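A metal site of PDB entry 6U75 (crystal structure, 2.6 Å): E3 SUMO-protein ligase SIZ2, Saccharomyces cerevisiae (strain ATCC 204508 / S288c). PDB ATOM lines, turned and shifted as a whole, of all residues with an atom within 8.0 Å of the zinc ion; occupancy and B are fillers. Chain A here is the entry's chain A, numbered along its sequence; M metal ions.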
ATOM      1  N   ALA A 198     -16.545 -10.407  -0.428  1.00  0.00           N
ATOM      2  CA  ALA A 198     -17.269  -9.441  -1.233  1.00  0.00           C
ATOM      3  C   ALA A 198     -16.307  -8.700  -2.150  1.00  0.00           C
ATOM      4  O   ALA A 198     -15.092  -8.723  -1.983  1.00  0.00           O
ATOM      5  CB  ALA A 198     -18.030  -8.433  -0.360  1.00  0.00           C
ATOM      6  N   LYS A 199     -16.902  -8.018  -3.137  1.00  0.00           N
ATOM      7  CA  LYS A 199     -16.171  -7.155  -4.051  1.00  0.00           C
ATOM      8  C   LYS A 199     -17.176  -6.368  -4.873  1.00  0.00           C
ATOM      9  O   LYS A 199     -18.328  -6.197  -4.440  1.00  0.00           O
ATOM     10  CB  LYS A 199     -15.238  -7.975  -4.954  1.00  0.00           C
ATOM     11  CG  LYS A 199     -15.939  -8.919  -5.915  1.00  0.00           C
ATOM     12  CD  LYS A 199     -14.939  -9.667  -6.780  1.00  0.00           C
ATOM     13  CE  LYS A 199     -15.633 -10.390  -7.918  1.00  0.00           C
ATOM     14  NZ  LYS A 199     -14.671 -11.114  -8.791  1.00  0.00           N
ATOM     15  N   THR A 200     -16.782  -5.880  -6.047  1.00  0.00           N
ATOM     16  CA  THR A 200     -17.685  -5.154  -6.919  1.00  0.00           C
ATOM     17  C   THR A 200     -17.601  -5.717  -8.335  1.00  0.00           C
ATOM     18  O   THR A 200     -16.597  -6.321  -8.718  1.00  0.00           O
ATOM     19  CB  THR A 200     -17.358  -3.649  -6.953  1.00  0.00           C
ATOM     20  OG1 THR A 200     -16.115  -3.444  -7.646  1.00  0.00           O
ATOM     21  CG2 THR A 200     -17.244  -3.099  -5.544  1.00  0.00           C
ATOM     22  N   GLN A 202     -17.230  -3.895 -10.699  1.00  0.00           N
ATOM     23  CA  GLN A 202     -16.225  -3.038 -11.310  1.00  0.00           C
ATOM     24  C   GLN A 202     -14.808  -3.546 -11.082  1.00  0.00           C
ATOM     25  O   GLN A 202     -13.876  -3.018 -11.693  1.00  0.00           O
ATOM     26  CB  GLN A 202     -16.344  -1.610 -10.774  1.00  0.00           C
ATOM     27  CG  GLN A 202     -17.749  -1.186 -10.360  1.00  0.00           C
ATOM     28  CD  GLN A 202     -18.774  -1.399 -11.452  1.00  0.00           C
ATOM     29  OE1 GLN A 202     -18.636  -0.889 -12.559  1.00  0.00           O
ATOM     30  NE2 GLN A 202     -19.818  -2.159 -11.140  1.00  0.00           N
ATOM     31  N   CYS A 203     -14.631  -4.540 -10.228  1.00  0.00           N
ATOM     32  CA  CYS A 203     -13.313  -5.048  -9.873  1.00  0.00           C
ATOM     33  C   CYS A 203     -12.875  -6.112 -10.871  1.00  0.00           C
ATOM     34  O   CYS A 203     -13.635  -7.052 -11.157  1.00  0.00           O
ATOM     35  CB  CYS A 203     -13.313  -5.611  -8.461  1.00  0.00           C
ATOM     36  SG  CYS A 203     -13.310  -4.360  -7.154  1.00  0.00           S
ATOM     37  N   LYS A 204     -11.660  -5.978 -11.385  1.00  0.00           N
ATOM     38  CA  LYS A 204     -11.115  -6.901 -12.372  1.00  0.00           C
ATOM     39  C   LYS A 204     -10.174  -7.896 -11.698  1.00  0.00           C
ATOM     40  O   LYS A 204      -8.982  -7.977 -12.003  1.00  0.00           O
ATOM     41  CB  LYS A 204     -10.406  -6.125 -13.482  1.00  0.00           C
ATOM     42  CG  LYS A 204     -11.192  -4.929 -14.016  1.00  0.00           C
ATOM     43  CD  LYS A 204     -12.464  -5.363 -14.734  1.00  0.00           C
ATOM     44  CE  LYS A 204     -13.461  -4.217 -14.836  1.00  0.00           C
ATOM     45  NZ  LYS A 204     -14.668  -4.596 -15.617  1.00  0.00           N
ATOM     46  N   HIS A 205     -10.732  -8.651 -10.761  1.00  0.00           N
ATOM     47  CA  HIS A 205      -9.963  -9.645 -10.015  1.00  0.00           C
ATOM     48  C   HIS A 205     -10.920 -10.568  -9.277  1.00  0.00           C
ATOM     49  O   HIS A 205     -11.971 -10.129  -8.818  1.00  0.00           O
ATOM     50  CB  HIS A 205      -8.992  -8.969  -9.028  1.00  0.00           C
ATOM     51  CG  HIS A 205      -9.650  -8.000  -8.096  1.00  0.00           C
ATOM     52  ND1 HIS A 205     -10.502  -8.405  -7.085  1.00  0.00           N
ATOM     53  CD2 HIS A 205      -9.584  -6.653  -8.014  1.00  0.00           C
ATOM     54  CE1 HIS A 205     -10.926  -7.346  -6.428  1.00  0.00           C
ATOM     55  NE2 HIS A 205     -10.380  -6.270  -6.962  1.00  0.00           N
ATOM     56  N   ILE A 206     -10.540 -11.843  -9.165  1.00  0.00           N
ATOM     57  CA  ILE A 206     -11.377 -12.808  -8.461  1.00  0.00           C
ATOM     58  C   ILE A 206     -11.177 -12.752  -6.950  1.00  0.00           C
ATOM     59  O   ILE A 206     -12.022 -13.265  -6.208  1.00  0.00           O
ATOM     60  CB  ILE A 206     -11.111 -14.242  -8.956  1.00  0.00           C
ATOM     61  CG1 ILE A 206      -9.621 -14.585  -8.839  1.00  0.00           C
ATOM     62  CG2 ILE A 206     -11.584 -14.411 -10.387  1.00  0.00           C
ATOM     63  CD1 ILE A 206      -9.328 -16.058  -9.024  1.00  0.00           C
ATOM     64  N   GLN A 207     -10.091 -12.150  -6.477  1.00  0.00           N
ATOM     65  CA  GLN A 207      -9.867 -12.056  -5.040  1.00  0.00           C
ATOM     66  C   GLN A 207     -10.926 -11.172  -4.389  1.00  0.00           C
ATOM     67  O   GLN A 207     -11.435 -10.225  -4.987  1.00  0.00           O
ATOM     68  CB  GLN A 207      -8.482 -11.501  -4.740  1.00  0.00           C
ATOM     69  CG  GLN A 207      -7.328 -12.419  -5.134  1.00  0.00           C
ATOM     70  CD  GLN A 207      -6.933 -12.264  -6.586  1.00  0.00           C
ATOM     71  OE1 GLN A 207      -7.724 -11.824  -7.424  1.00  0.00           O
ATOM     72  NE2 GLN A 207      -5.696 -12.624  -6.901  1.00  0.00           N
ATOM     73  N   CYS A 208     -11.261 -11.498  -3.140  1.00  0.00           N
ATOM     74  CA  CYS A 208     -12.306 -10.811  -2.388  1.00  0.00           C
ATOM     75  C   CYS A 208     -11.721 -10.318  -1.071  1.00  0.00           C
ATOM     76  O   CYS A 208     -10.577 -10.593  -0.716  1.00  0.00           O
ATOM     77  CB  CYS A 208     -13.508 -11.727  -2.147  1.00  0.00           C
ATOM     78  SG  CYS A 208     -14.300 -12.332  -3.640  1.00  0.00           S
ATOM     79  N   PHE A 209     -12.560  -9.581  -0.329  1.00  0.00           N
ATOM     80  CA  PHE A 209     -12.221  -9.106   0.997  1.00  0.00           C
ATOM     81  C   PHE A 209     -13.459  -9.209   1.879  1.00  0.00           C
ATOM     82  O   PHE A 209     -14.587  -9.119   1.397  1.00  0.00           O
ATOM     83  CB  PHE A 209     -11.728  -7.648   0.949  1.00  0.00           C
ATOM     84  CG  PHE A 209     -12.660  -6.715   0.239  1.00  0.00           C
ATOM     85  CD1 PHE A 209     -12.552  -6.517  -1.119  1.00  0.00           C
ATOM     86  CD2 PHE A 209     -13.650  -6.044   0.937  1.00  0.00           C
ATOM     87  CE1 PHE A 209     -13.411  -5.663  -1.785  1.00  0.00           C
ATOM     88  CE2 PHE A 209     -14.511  -5.183   0.278  1.00  0.00           C
ATOM     89  CZ  PHE A 209     -14.392  -4.993  -1.082  1.00  0.00           C
ATOM     90  N   GLN A 225     -11.607   2.722  -1.113  1.00  0.00           N
ATOM     91  CA  GLN A 225     -10.804   2.133  -2.175  1.00  0.00           C
ATOM     92  C   GLN A 225     -10.705   0.637  -1.935  1.00  0.00           C
ATOM     93  O   GLN A 225     -10.500   0.187  -0.802  1.00  0.00           O
ATOM     94  CB  GLN A 225      -9.406   2.748  -2.222  1.00  0.00           C
ATOM     95  CG  GLN A 225      -9.400   4.246  -2.502  1.00  0.00           C
ATOM     96  CD  GLN A 225      -8.022   4.846  -2.381  1.00  0.00           C
ATOM     97  OE1 GLN A 225      -7.017   4.129  -2.358  1.00  0.00           O
ATOM     98  NE2 GLN A 225      -7.959   6.172  -2.293  1.00  0.00           N
ATOM     99  N   CYS A 226     -10.867  -0.140  -3.000  1.00  0.00           N
ATOM    100  CA  CYS A 226     -10.773  -1.579  -2.892  1.00  0.00           C
ATOM    101  C   CYS A 226      -9.435  -1.961  -2.248  1.00  0.00           C
ATOM    102  O   CYS A 226      -8.376  -1.521  -2.715  1.00  0.00           O
ATOM    103  CB  CYS A 226     -10.887  -2.230  -4.271  1.00  0.00           C
ATOM    104  SG  CYS A 226     -10.752  -4.028  -4.284  1.00  0.00           S
ATOM    105  N   PRO A 227      -9.432  -2.777  -1.180  1.00  0.00           N
ATOM    106  CA  PRO A 227      -8.167  -3.161  -0.545  1.00  0.00           C
ATOM    107  C   PRO A 227      -7.230  -3.959  -1.453  1.00  0.00           C
ATOM    108  O   PRO A 227      -6.120  -4.286  -1.030  1.00  0.00           O
ATOM    109  CB  PRO A 227      -8.606  -4.009   0.656  1.00  0.00           C
ATOM    110  CG  PRO A 227     -10.051  -3.707   0.858  1.00  0.00           C
ATOM    111  CD  PRO A 227     -10.588  -3.393  -0.497  1.00  0.00           C
ATOM    112  N   ILE A 228      -7.655  -4.292  -2.675  1.00  0.00           N
ATOM    113  CA  ILE A 228      -6.867  -5.100  -3.594  1.00  0.00           C
ATOM    114  C   ILE A 228      -6.383  -4.270  -4.776  1.00  0.00           C
ATOM    115  O   ILE A 228      -5.187  -4.149  -5.021  1.00  0.00           O
ATOM    116  CB  ILE A 228      -7.657  -6.341  -4.054  1.00  0.00           C
ATOM    117  CG1 ILE A 228      -8.102  -7.155  -2.832  1.00  0.00           C
ATOM    118  CG2 ILE A 228      -6.825  -7.187  -5.008  1.00  0.00           C
ATOM    119  CD1 ILE A 228      -8.972  -8.340  -3.170  1.00  0.00           C
ATOM    120  N   CYS A 229      -7.315  -3.683  -5.533  1.00  0.00           N
ATOM    121  CA  CYS A 229      -6.990  -2.905  -6.715  1.00  0.00           C
ATOM    122  C   CYS A 229      -6.967  -1.401  -6.471  1.00  0.00           C
ATOM    123  O   CYS A 229      -6.571  -0.644  -7.362  1.00  0.00           O
ATOM    124  CB  CYS A 229      -7.987  -3.217  -7.844  1.00  0.00           C
ATOM    125  SG  CYS A 229      -9.703  -2.821  -7.448  1.00  0.00           S
ATOM    126  N   GLN A 230      -7.385  -0.944  -5.293  1.00  0.00           N
ATOM    127  CA  GLN A 230      -7.381   0.462  -4.898  1.00  0.00           C
ATOM    128  C   GLN A 230      -8.283   1.330  -5.767  1.00  0.00           C
ATOM    129  O   GLN A 230      -8.230   2.563  -5.678  1.00  0.00           O
ATOM    130  CB  GLN A 230      -5.957   1.038  -4.913  1.00  0.00           C
ATOM    131  CG  GLN A 230      -5.278   0.984  -3.552  1.00  0.00           C
ATOM    132  CD  GLN A 230      -5.130  -0.431  -3.028  1.00  0.00           C
ATOM    133  OE1 GLN A 230      -5.075  -1.388  -3.795  1.00  0.00           O
ATOM    134  NE2 GLN A 230      -5.096  -0.574  -1.708  1.00  0.00           N
ATOM    135  N   HIS A 231      -9.109   0.729  -6.620  1.00  0.00           N
ATOM    136  CA  HIS A 231     -10.081   1.524  -7.366  1.00  0.00           C
ATOM    137  C   HIS A 231     -11.099   2.134  -6.412  1.00  0.00           C
ATOM    138  O   HIS A 231     -11.498   1.493  -5.436  1.00  0.00           O
ATOM    139  CB  HIS A 231     -10.794   0.670  -8.408  1.00  0.00           C
ATOM    140  CG  HIS A 231     -10.101   0.613  -9.736  1.00  0.00           C
ATOM    141  ND1 HIS A 231      -9.380  -0.487 -10.151  1.00  0.00           N
ATOM    142  CD2 HIS A 231     -10.017   1.518 -10.734  1.00  0.00           C
ATOM    143  CE1 HIS A 231      -8.886  -0.252 -11.358  1.00  0.00           C
ATOM    144  NE2 HIS A 231      -9.257   0.957 -11.736  1.00  0.00           N
ATOM    145  N   PRO A 232     -11.526   3.376  -6.652  1.00  0.00           N
ATOM    146  CA  PRO A 232     -12.573   3.964  -5.788  1.00  0.00           C
ATOM    147  C   PRO A 232     -13.901   3.273  -6.020  1.00  0.00           C
ATOM    148  O   PRO A 232     -14.406   3.225  -7.147  1.00  0.00           O
ATOM    149  CB  PRO A 232     -12.605   5.431  -6.239  1.00  0.00           C
ATOM    150  CG  PRO A 232     -12.118   5.406  -7.639  1.00  0.00           C
ATOM    151  CD  PRO A 232     -11.088   4.309  -7.706  1.00  0.00           C
ATOM    152  N   ILE A 233     -14.473   2.718  -4.954  1.00  0.00           N
ATOM    153  CA  ILE A 233     -15.755   2.043  -5.012  1.00  0.00           C
ATOM    154  C   ILE A 233     -16.718   2.749  -4.063  1.00  0.00           C
ATOM    155  O   ILE A 233     -16.347   3.656  -3.306  1.00  0.00           O
ATOM    156  CB  ILE A 233     -15.643   0.548  -4.651  1.00  0.00           C
ATOM    157  CG1 ILE A 233     -14.987   0.367  -3.288  1.00  0.00           C
ATOM    158  CG2 ILE A 233     -14.856  -0.189  -5.731  1.00  0.00           C
ATOM    159  CD1 ILE A 233     -14.949  -1.073  -2.819  1.00  0.00           C
HETATM  160 ZN    ZN M   1     -11.092  -4.403  -6.556  1.00  0.00          ZN
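Within 4 Å of the zinc ion: Cys 203, His 205, Cys 226 and Cys 229.
The side-chain amino group of Lys 199 is in hydrogen-bond range of the backbone carbonyl oxygen of His 205. A ring nitrogen (ND1) of His 205 sits at hydrogen-bond distance from the backbone carbonyl oxygen of Gln 207, 2.9 Å away. A ring nitrogen (ND1) of His 231 sits close to the side-chain sulfur (SG) of Cys 229 (3.6 Å). N of Cys 203 sits at hydrogen-bond distance from OG1 of Thr 200 (3.2 Å). The backbone NH (N) of Ile 228 sits close to the side-chain sulfur (SG) of Cys 226, at 3.5 Å. O of Cys 226 lies close to OE1 of Gln 230 (3.5 Å). The backbone NH (N) of Cys 226 sits at hydrogen-bond distance from the backbone carbonyl oxygen (O) of His 231 (3.0 Å).
The zinc ion is bound by NE2 of His 205, SG of Cys 229, SG of Cys 203 and SG of Cys 226. The zinc ion has four donor atoms within binding distance.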
